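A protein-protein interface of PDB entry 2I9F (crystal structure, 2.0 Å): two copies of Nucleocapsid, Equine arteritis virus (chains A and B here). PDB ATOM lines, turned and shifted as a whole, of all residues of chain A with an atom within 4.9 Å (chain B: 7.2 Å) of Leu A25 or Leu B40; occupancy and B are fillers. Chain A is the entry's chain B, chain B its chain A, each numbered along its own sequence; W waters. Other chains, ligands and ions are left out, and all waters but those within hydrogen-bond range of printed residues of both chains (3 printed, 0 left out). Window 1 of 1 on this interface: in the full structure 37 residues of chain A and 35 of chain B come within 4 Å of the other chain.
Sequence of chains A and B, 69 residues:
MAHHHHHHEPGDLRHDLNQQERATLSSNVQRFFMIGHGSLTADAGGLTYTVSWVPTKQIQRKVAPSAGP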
ATOM      1  N   ASP A  12       9.381   5.644  28.151  1.00  0.00           N
ATOM      2  CA  ASP A  12       8.560   4.823  29.042  1.00  0.00           C
ATOM      3  C   ASP A  12       9.476   4.083  30.012  1.00  0.00           C
ATOM      4  O   ASP A  12      10.655   4.488  30.223  1.00  0.00           O
ATOM      5  CB  ASP A  12       7.558   3.893  28.277  1.00  0.00           C
ATOM      6  CG  ASP A  12       8.225   2.925  27.372  1.00  0.00           C
ATOM      7  OD1 ASP A  12       9.451   2.693  27.487  1.00  0.00           O
ATOM      8  OD2 ASP A  12       7.514   2.323  26.541  1.00  0.00           O
ATOM      9  N   LEU A  13       8.984   2.985  30.589  1.00  0.00           N
ATOM     10  CA  LEU A  13       9.769   2.308  31.594  1.00  0.00           C
ATOM     11  C   LEU A  13      11.115   1.786  31.060  1.00  0.00           C
ATOM     12  O   LEU A  13      12.040   1.581  31.858  1.00  0.00           O
ATOM     13  CB  LEU A  13       8.962   1.223  32.307  1.00  0.00           C
ATOM     14  CG  LEU A  13       7.850   1.773  33.239  1.00  0.00           C
ATOM     15  CD1 LEU A  13       7.198   0.654  33.974  1.00  0.00           C
ATOM     16  CD2 LEU A  13       8.316   2.843  34.266  1.00  0.00           C
ATOM     17  N   ARG A  14      11.253   1.577  29.743  1.00  0.00           N
ATOM     18  CA  ARG A  14      12.563   1.187  29.225  1.00  0.00           C
ATOM     19  C   ARG A  14      13.646   2.265  29.426  1.00  0.00           C
ATOM     20  O   ARG A  14      14.811   1.944  29.501  1.00  0.00           O
ATOM     21  CB  ARG A  14      12.514   0.793  27.760  1.00  0.00           C
ATOM     22  CG  ARG A  14      11.654  -0.460  27.484  1.00  0.00           C
ATOM     23  CD  ARG A  14      11.439  -0.638  26.053  1.00  0.00           C
ATOM     24  NE  ARG A  14      10.244   0.093  25.679  1.00  0.00           N
ATOM     25  CZ  ARG A  14       9.585  -0.030  24.538  1.00  0.00           C
ATOM     26  NH1 ARG A  14       8.516   0.725  24.325  1.00  0.00           N
ATOM     27  NH2 ARG A  14      10.033  -0.821  23.580  1.00  0.00           N
ATOM     28  N   LEU A  17      15.931   1.435  32.380  1.00  0.00           N
ATOM     29  CA  LEU A  17      16.520   0.113  32.407  1.00  0.00           C
ATOM     30  C   LEU A  17      17.739   0.040  31.543  1.00  0.00           C
ATOM     31  O   LEU A  17      17.801   0.701  30.497  1.00  0.00           O
ATOM     32  CB  LEU A  17      15.482  -0.934  31.944  1.00  0.00           C
ATOM     33  CG  LEU A  17      14.221  -0.918  32.789  1.00  0.00           C
ATOM     34  CD1 LEU A  17      13.175  -1.959  32.264  1.00  0.00           C
ATOM     35  CD2 LEU A  17      14.567  -1.145  34.254  1.00  0.00           C
ATOM     36  N   GLU A  21      18.726  -5.539  31.394  1.00  0.00           N
ATOM     37  CA  GLU A  21      17.360  -5.480  31.901  1.00  0.00           C
ATOM     38  C   GLU A  21      16.305  -5.392  30.780  1.00  0.00           C
ATOM     39  O   GLU A  21      15.347  -6.171  30.761  1.00  0.00           O
ATOM     40  CB  GLU A  21      17.243  -4.321  32.861  1.00  0.00           C
ATOM     41  CG  GLU A  21      17.881  -4.605  34.231  1.00  0.00           C
ATOM     42  CD  GLU A  21      18.096  -3.363  35.022  1.00  0.00           C
ATOM     43  OE1 GLU A  21      18.022  -2.256  34.408  1.00  0.00           O
ATOM     44  OE2 GLU A  21      18.293  -3.492  36.249  1.00  0.00           O
ATOM     45  N   ARG A  22      16.461  -4.434  29.880  1.00  0.00           N
ATOM     46  CA  ARG A  22      15.668  -4.414  28.651  1.00  0.00           C
ATOM     47  C   ARG A  22      15.728  -5.778  27.889  1.00  0.00           C
ATOM     48  O   ARG A  22      14.687  -6.303  27.489  1.00  0.00           O
ATOM     49  CB  ARG A  22      16.105  -3.259  27.738  1.00  0.00           C
ATOM     50  CG  ARG A  22      15.722  -1.845  28.227  1.00  0.00           C
ATOM     51  CD  ARG A  22      16.686  -0.744  27.622  1.00  0.00           C
ATOM     52  NE  ARG A  22      16.596  -0.787  26.172  1.00  0.00           N
ATOM     53  CZ  ARG A  22      17.602  -0.929  25.306  1.00  0.00           C
ATOM     54  NH1 ARG A  22      18.889  -1.000  25.696  1.00  0.00           N
ATOM     55  NH2 ARG A  22      17.297  -0.986  24.013  1.00  0.00           N
ATOM     56  N   ALA A  23      16.916  -6.374  27.731  1.00  0.00           N
ATOM     57  CA  ALA A  23      16.989  -7.699  27.075  1.00  0.00           C
ATOM     58  C   ALA A  23      16.243  -8.858  27.860  1.00  0.00           C
ATOM     59  O   ALA A  23      15.560  -9.706  27.256  1.00  0.00           O
ATOM     60  CB  ALA A  23      18.430  -8.060  26.802  1.00  0.00           C
ATOM     61  N   THR A  24      16.394  -8.902  29.176  1.00  0.00           N
ATOM     62  CA  THR A  24      15.545  -9.769  30.033  1.00  0.00           C
ATOM     63  C   THR A  24      14.031  -9.566  29.748  1.00  0.00           C
ATOM     64  O   THR A  24      13.312 -10.532  29.474  1.00  0.00           O
ATOM     65  CB  THR A  24      15.795  -9.500  31.527  1.00  0.00           C
ATOM     66  OG1 THR A  24      17.152  -9.836  31.811  1.00  0.00           O
ATOM     67  CG2 THR A  24      14.862 -10.358  32.395  1.00  0.00           C
ATOM     68  N   LEU A  25      13.567  -8.323  29.802  1.00  0.00           N
ATOM     69  CA  LEU A  25      12.147  -8.051  29.450  1.00  0.00           C
ATOM     70  C   LEU A  25      11.712  -8.391  28.023  1.00  0.00           C
ATOM     71  O   LEU A  25      10.595  -8.875  27.833  1.00  0.00           O
ATOM     72  CB  LEU A  25      11.765  -6.623  29.816  1.00  0.00           C
ATOM     73  CG  LEU A  25      11.847  -6.197  31.295  1.00  0.00           C
ATOM     74  CD1 LEU A  25      11.363  -4.772  31.387  1.00  0.00           C
ATOM     75  CD2 LEU A  25      11.044  -7.126  32.251  1.00  0.00           C
ATOM     76  N   SER A  26      12.554  -8.099  27.022  1.00  0.00           N
ATOM     77  CA  SER A  26      12.276  -8.541  25.630  1.00  0.00           C
ATOM     78  C   SER A  26      12.067 -10.047  25.528  1.00  0.00           C
ATOM     79  O   SER A  26      11.177 -10.547  24.844  1.00  0.00           O
ATOM     80  CB  SER A  26      13.377  -8.060  24.682  1.00  0.00           C
ATOM     81  OG  SER A  26      14.497  -8.932  24.763  1.00  0.00           O
ATOM     82  N   SER A  27      12.864 -10.786  26.282  1.00  0.00           N
ATOM     83  CA  SER A  27      12.794 -12.231  26.334  1.00  0.00           C
ATOM     84  C   SER A  27      11.536 -12.735  27.019  1.00  0.00           C
ATOM     85  O   SER A  27      10.939 -13.741  26.571  1.00  0.00           O
ATOM     86  CB  SER A  27      14.069 -12.789  26.997  1.00  0.00           C
ATOM     87  OG  SER A  27      13.910 -14.158  27.139  1.00  0.00           O
ATOM     88  N   ASN A  28      11.140 -12.038  28.094  1.00  0.00           N
ATOM     89  CA  ASN A  28       9.903 -12.325  28.822  1.00  0.00           C
ATOM     90  C   ASN A  28       8.752 -12.225  27.807  1.00  0.00           C
ATOM     91  O   ASN A  28       7.965 -13.149  27.667  1.00  0.00           O
ATOM     92  CB  ASN A  28       9.656 -11.306  29.963  1.00  0.00           C
ATOM     93  CG  ASN A  28      10.527 -11.542  31.200  1.00  0.00           C
ATOM     94  OD1 ASN A  28      11.147 -12.593  31.387  1.00  0.00           O
ATOM     95  ND2 ASN A  28      10.585 -10.550  32.031  1.00  0.00           N
ATOM     96  N   VAL A  29       8.685 -11.122  27.078  1.00  0.00           N
ATOM     97  CA  VAL A  29       7.581 -10.862  26.131  1.00  0.00           C
ATOM     98  C   VAL A  29       7.554 -11.950  25.047  1.00  0.00           C
ATOM     99  O   VAL A  29       6.494 -12.365  24.587  1.00  0.00           O
ATOM    100  CB  VAL A  29       7.710  -9.393  25.485  1.00  0.00           C
ATOM    101  CG1 VAL A  29       6.766  -9.203  24.319  1.00  0.00           C
ATOM    102  CG2 VAL A  29       7.373  -8.317  26.550  1.00  0.00           C
ATOM    103  N   TRP A  53       2.583  -8.574  33.280  1.00  0.00           N
ATOM    104  CA  TRP A  53       3.328  -9.487  34.128  1.00  0.00           C
ATOM    105  C   TRP A  53       4.080  -8.723  35.169  1.00  0.00           C
ATOM    106  O   TRP A  53       4.299  -7.508  35.017  1.00  0.00           O
ATOM    107  CB  TRP A  53       4.341 -10.317  33.307  1.00  0.00           C
ATOM    108  CG  TRP A  53       5.626  -9.709  32.806  1.00  0.00           C
ATOM    109  CD1 TRP A  53       6.902 -10.058  33.207  1.00  0.00           C
ATOM    110  CD2 TRP A  53       5.792  -8.758  31.745  1.00  0.00           C
ATOM    111  NE1 TRP A  53       7.822  -9.361  32.481  1.00  0.00           N
ATOM    112  CE2 TRP A  53       7.167  -8.551  31.586  1.00  0.00           C
ATOM    113  CE3 TRP A  53       4.892  -8.035  30.927  1.00  0.00           C
ATOM    114  CZ2 TRP A  53       7.697  -7.667  30.614  1.00  0.00           C
ATOM    115  CZ3 TRP A  53       5.408  -7.124  29.997  1.00  0.00           C
ATOM    116  CH2 TRP A  53       6.798  -6.964  29.826  1.00  0.00           C
ATOM    117  N   PRO A  55       7.762  -8.499  36.556  1.00  0.00           N
ATOM    118  CA  PRO A  55       9.060  -8.973  36.149  1.00  0.00           C
ATOM    119  C   PRO A  55       9.891  -9.460  37.370  1.00  0.00           C
ATOM    120  O   PRO A  55       9.495  -9.265  38.524  1.00  0.00           O
ATOM    121  CB  PRO A  55       9.681  -7.706  35.521  1.00  0.00           C
ATOM    122  CG  PRO A  55       9.201  -6.636  36.394  1.00  0.00           C
ATOM    123  CD  PRO A  55       7.721  -7.026  36.585  1.00  0.00           C
ATOM    124  N   ILE A  59      14.142  -6.092  38.525  1.00  0.00           N
ATOM    125  CA  ILE A  59      13.509  -5.129  37.631  1.00  0.00           C
ATOM    126  C   ILE A  59      12.286  -4.538  38.274  1.00  0.00           C
ATOM    127  O   ILE A  59      12.014  -3.340  38.128  1.00  0.00           O
ATOM    128  CB  ILE A  59      13.198  -5.775  36.297  1.00  0.00           C
ATOM    129  CG1 ILE A  59      14.531  -6.033  35.554  1.00  0.00           C
ATOM    130  CG2 ILE A  59      12.255  -4.892  35.473  1.00  0.00           C
ATOM    131  CD1 ILE A  59      14.367  -6.863  34.259  1.00  0.00           C
ATOM    132  N   GLN B  30       9.682  -9.415  20.265  1.00  0.00           N
ATOM    133  CA  GLN B  30      10.971  -9.261  20.940  1.00  0.00           C
ATOM    134  C   GLN B  30      11.827  -8.104  20.369  1.00  0.00           C
ATOM    135  O   GLN B  30      12.390  -7.271  21.113  1.00  0.00           O
ATOM    136  CB  GLN B  30      11.762 -10.551  20.848  1.00  0.00           C
ATOM    137  CG  GLN B  30      13.094 -10.439  21.643  1.00  0.00           C
ATOM    138  CD  GLN B  30      13.750 -11.765  21.932  1.00  0.00           C
ATOM    139  OE1 GLN B  30      13.884 -12.608  21.037  1.00  0.00           O
ATOM    140  NE2 GLN B  30      14.222 -11.949  23.164  1.00  0.00           N
ATOM    141  N   PHE B  33      10.470  -4.622  21.055  1.00  0.00           N
ATOM    142  CA  PHE B  33      10.716  -4.222  22.431  1.00  0.00           C
ATOM    143  C   PHE B  33      12.109  -3.612  22.474  1.00  0.00           C
ATOM    144  O   PHE B  33      12.321  -2.506  23.032  1.00  0.00           O
ATOM    145  CB  PHE B  33      10.645  -5.433  23.407  1.00  0.00           C
ATOM    146  CG  PHE B  33      10.727  -5.027  24.853  1.00  0.00           C
ATOM    147  CD1 PHE B  33       9.575  -4.881  25.596  1.00  0.00           C
ATOM    148  CD2 PHE B  33      11.952  -4.707  25.452  1.00  0.00           C
ATOM    149  CE1 PHE B  33       9.601  -4.473  26.927  1.00  0.00           C
ATOM    150  CE2 PHE B  33      12.012  -4.319  26.796  1.00  0.00           C
ATOM    151  CZ  PHE B  33      10.843  -4.192  27.531  1.00  0.00           C
ATOM    152  N   MET B  34      13.054  -4.303  21.841  1.00  0.00           N
ATOM    153  CA  MET B  34      14.462  -3.823  21.843  1.00  0.00           C
ATOM    154  C   MET B  34      14.719  -2.538  21.076  1.00  0.00           C
ATOM    155  O   MET B  34      15.633  -1.812  21.413  1.00  0.00           O
ATOM    156  CB  MET B  34      15.446  -4.905  21.375  1.00  0.00           C
ATOM    157  CG  MET B  34      15.475  -6.098  22.274  1.00  0.00           C
ATOM    158  SD  MET B  34      15.997  -5.624  24.146  1.00  0.00           S
ATOM    159  CE  MET B  34      17.828  -4.802  23.877  1.00  0.00           C
ATOM    160  N   HIS B  37       9.871   0.323  20.170  1.00  0.00           N
ATOM    161  CA  HIS B  37       8.503   0.445  19.623  1.00  0.00           C
ATOM    162  C   HIS B  37       7.543  -0.110  20.696  1.00  0.00           C
ATOM    163  O   HIS B  37       7.973  -0.898  21.564  1.00  0.00           O
ATOM    164  CB  HIS B  37       8.358  -0.307  18.277  1.00  0.00           C
ATOM    165  CG  HIS B  37       7.205   0.169  17.409  1.00  0.00           C
ATOM    166  ND1 HIS B  37       7.107   1.463  16.918  1.00  0.00           N
ATOM    167  CD2 HIS B  37       6.112  -0.483  16.921  1.00  0.00           C
ATOM    168  CE1 HIS B  37       6.008   1.584  16.179  1.00  0.00           C
ATOM    169  NE2 HIS B  37       5.388   0.419  16.164  1.00  0.00           N
ATOM    170  N   GLY B  38       6.280   0.263  20.626  1.00  0.00           N
ATOM    171  CA  GLY B  38       5.262  -0.178  21.579  1.00  0.00           C
ATOM    172  C   GLY B  38       5.327   0.677  22.857  1.00  0.00           C
ATOM    173  O   GLY B  38       6.080   1.705  22.968  1.00  0.00           O
ATOM    174  N   SER B  39       4.586   0.247  23.853  1.00  0.00           N
ATOM    175  CA  SER B  39       4.485   1.034  25.076  1.00  0.00           C
ATOM    176  C   SER B  39       4.693   0.106  26.261  1.00  0.00           C
ATOM    177  O   SER B  39       3.990  -0.906  26.348  1.00  0.00           O
ATOM    178  CB  SER B  39       3.098   1.662  25.189  1.00  0.00           C
ATOM    179  OG  SER B  39       3.070   2.473  26.373  1.00  0.00           O
ATOM    180  N   LEU B  40       5.650   0.457  27.146  1.00  0.00           N
ATOM    181  CA  LEU B  40       5.913  -0.320  28.377  1.00  0.00           C
ATOM    182  C   LEU B  40       5.539   0.551  29.584  1.00  0.00           C
ATOM    183  O   LEU B  40       6.158   1.546  29.869  1.00  0.00           O
ATOM    184  CB  LEU B  40       7.332  -0.912  28.469  1.00  0.00           C
ATOM    185  CG  LEU B  40       7.558  -1.715  29.756  1.00  0.00           C
ATOM    186  CD1 LEU B  40       6.906  -3.105  29.657  1.00  0.00           C
ATOM    187  CD2 LEU B  40       9.020  -1.816  30.115  1.00  0.00           C
ATOM    188  N   THR B  41       4.450   0.189  30.229  1.00  0.00           N
ATOM    189  CA  THR B  41       3.961   0.952  31.371  1.00  0.00           C
ATOM    190  C   THR B  41       3.814   0.074  32.611  1.00  0.00           C
ATOM    191  O   THR B  41       3.755  -1.165  32.540  1.00  0.00           O
ATOM    192  CB  THR B  41       2.567   1.569  31.091  1.00  0.00           C
ATOM    193  OG1 THR B  41       1.684   0.534  30.695  1.00  0.00           O
ATOM    194  CG2 THR B  41       2.610   2.629  30.002  1.00  0.00           C
ATOM    195  N   ALA B  42       3.674   0.771  33.743  1.00  0.00           N
ATOM    196  CA  ALA B  42       3.577   0.180  35.064  1.00  0.00           C
ATOM    197  C   ALA B  42       2.112   0.104  35.354  1.00  0.00           C
ATOM    198  O   ALA B  42       1.444   1.127  35.437  1.00  0.00           O
ATOM    199  CB  ALA B  42       4.265   1.081  36.080  1.00  0.00           C
ATOM    200  N   LEU B  47       3.923  -4.807  34.969  1.00  0.00           N
ATOM    201  CA  LEU B  47       4.241  -4.169  33.726  1.00  0.00           C
ATOM    202  C   LEU B  47       3.144  -4.537  32.718  1.00  0.00           C
ATOM    203  O   LEU B  47       2.545  -5.589  32.833  1.00  0.00           O
ATOM    204  CB  LEU B  47       5.601  -4.687  33.223  1.00  0.00           C
ATOM    205  CG  LEU B  47       6.813  -4.151  33.988  1.00  0.00           C
ATOM    206  CD1 LEU B  47       8.091  -4.815  33.430  1.00  0.00           C
ATOM    207  CD2 LEU B  47       6.940  -2.619  33.860  1.00  0.00           C
ATOM    208  N   THR B  48       2.858  -3.638  31.788  1.00  0.00           N
ATOM    209  CA  THR B  48       2.151  -4.037  30.592  1.00  0.00           C
ATOM    210  C   THR B  48       2.946  -3.566  29.421  1.00  0.00           C
ATOM    211  O   THR B  48       3.381  -2.399  29.390  1.00  0.00           O
ATOM    212  CB  THR B  48       0.700  -3.495  30.571  1.00  0.00           C
ATOM    213  OG1 THR B  48       0.022  -4.058  31.686  1.00  0.00           O
ATOM    214  CG2 THR B  48      -0.077  -3.856  29.250  1.00  0.00           C
ATOM    215  N   TYR B  49       3.159  -4.493  28.492  1.00  0.00           N
ATOM    216  CA  TYR B  49       3.727  -4.155  27.196  1.00  0.00           C
ATOM    217  C   TYR B  49       2.682  -4.312  26.077  1.00  0.00           C
ATOM    218  O   TYR B  49       2.000  -5.338  25.961  1.00  0.00           O
ATOM    219  CB  TYR B  49       5.007  -4.971  26.895  1.00  0.00           C
ATOM    220  CG  TYR B  49       5.662  -4.572  25.540  1.00  0.00           C
ATOM    221  CD1 TYR B  49       6.253  -3.323  25.379  1.00  0.00           C
ATOM    222  CD2 TYR B  49       5.609  -5.440  24.424  1.00  0.00           C
ATOM    223  CE1 TYR B  49       6.819  -2.928  24.149  1.00  0.00           C
ATOM    224  CE2 TYR B  49       6.141  -5.063  23.179  1.00  0.00           C
ATOM    225  CZ  TYR B  49       6.800  -3.803  23.085  1.00  0.00           C
ATOM    226  OH  TYR B  49       7.349  -3.434  21.918  1.00  0.00           O
ATOM    227  N   THR B  50       2.570  -3.296  25.242  1.00  0.00           N
ATOM    228  CA  THR B  50       1.647  -3.387  24.128  1.00  0.00           C
ATOM    229  C   THR B  50       2.326  -2.871  22.865  1.00  0.00           C
ATOM    230  O   THR B  50       3.126  -1.904  22.900  1.00  0.00           O
ATOM    231  CB  THR B  50       0.236  -2.716  24.423  1.00  0.00           C
ATOM    232  OG1 THR B  50      -0.630  -2.928  23.278  1.00  0.00           O
ATOM    233  CG2 THR B  50       0.349  -1.253  24.704  1.00  0.00           C
HETATM  234  O   HOH W   1      14.320  -1.596  24.796  1.00  0.00           O
HETATM  235  O   HOH W   2      14.568 -14.340  24.117  1.00  0.00           O
HETATM  236  O   HOH W   3      15.649   1.253  22.063  1.00  0.00           O
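OG of Ser A26 sits at hydrogen-bond distance from NE2 of Gln B30 (3.4 Å).
NH2 of Arg A14 sits at hydrogen-bond distance from O of Phe B33 (2.9 Å).
O of Met B34 is in hydrogen-bond range of NH2 of Arg A22.
The backbone NH (N) of Ala A23 sits close to the side-chain sulfur (SD) of Met B34, 3.8 Å away.
The side-chain sulfur of Met B34 lies close to the side-chain hydroxyl of Ser A26 (3.7 Å).
O of His B37 is in hydrogen-bond range of NH2 of Arg A14 (2.9 Å).
O of Gly B38 sits at hydrogen-bond distance from NH1 of Arg A14.
The backbone NH (N) of Leu B40 is in hydrogen-bond range of the side-chain carboxylate (OD2) of Asp A12 (2.7 Å).
O of Leu B40 is in hydrogen-bond range of N of Leu A13, 3.3 Å away.
The backbone NH (N) of Leu B47 is in hydrogen-bond range of the backbone carbonyl oxygen (O) of Trp A53, at 2.7 Å.
O of His B37 lies within hydrogen-bond range of OH of Tyr B49, at 2.6 Å.
The backbone carbonyl oxygen (O) of Thr B50 lies within hydrogen-bond range of the backbone NH (N) of Ser B39, 2.8 Å away.
The backbone NH of Thr B48 is in hydrogen-bond range of the backbone carbonyl oxygen of Thr B41 (2.7 Å).
The guanidinium group (NH1) of Arg A14 is in salt-bridge range of the side-chain carboxylate (OD2) of Asp A12, at 2.9 Å.
O of Ala A23 sits at hydrogen-bond distance from OG of Ser A26 (2.8 Å).
The side-chain amide nitrogen (ND2) of Asn A28 lies close to the indole nitrogen (NE1) of Trp A53 (3.0 Å).
Leu A13 touches Leu B47.
Arg A14 touches Ser B39 (NH1 to N, 3.99 Å).
Arg A14 touches Leu B40.
Arg A22 touches Phe B33.
CD1 of Leu A25 touches CD2 of Leu B40 (3.98 Å).
Leu A25 touches Leu B47 (CD1 to CD1, 3.9 Å).
Val A29 touches Tyr B49 (CG1 to CD2, 3.9 Å).
CH2 of Trp A53 touches CD1 of Leu B40, at 3.9 Å.
Trp A53 touches Tyr B49.
CG of Pro A55 touches CD1 of Leu B47, 3.7 Å away.
Printed residues of chain B within 4 Å of Leu A25: Phe B33 (3.5 Å), Leu B40 (3.98 Å) and Leu B47 (3.9 Å).
Of the printed residues of chain A, Leu B40 touches Asp A12 (2.7 Å), Leu A13 (3.3 Å), Arg A14 (3.96 Å), Leu A25 (3.98 Å) and Trp A53 (3.9 Å).
Of the printed residues of chain B, Asp A12 touches Gly B38 (3.9 Å), Ser B39 (3.6 Å) and Leu B40 (2.7 Å).
Printed residues of chain B within 4 Å of Ala A23: Met B34 (3.7 Å).
The nearest printed residue of chain B that does not touch Pro A55 is Thr B48 (7.6 Å).
Hydrophobic or aromatic side chains of chain A within 4 Å of the printed part of chain B: Leu A13, Leu A25, Val A29, Trp A53 and Pro A55.
Of the 13 printed residues of chain B, 11 touch a printed residue of chain A.
No position is printed for both chains.
Water W2 lies within hydrogen-bond range of the side-chain amide nitrogen of Gln B30 (2.6 Å) and the side-chain hydroxyl of Ser A27 (3.1 Å).
Water W1 bridges NE of Arg A22 (2.8 Å) and O of Phe B33 (2.8 Å).
Water W3 lies within hydrogen-bond range of the backbone carbonyl oxygen (O) of Met B34 and the guanidinium group (NH2) of Arg A22.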
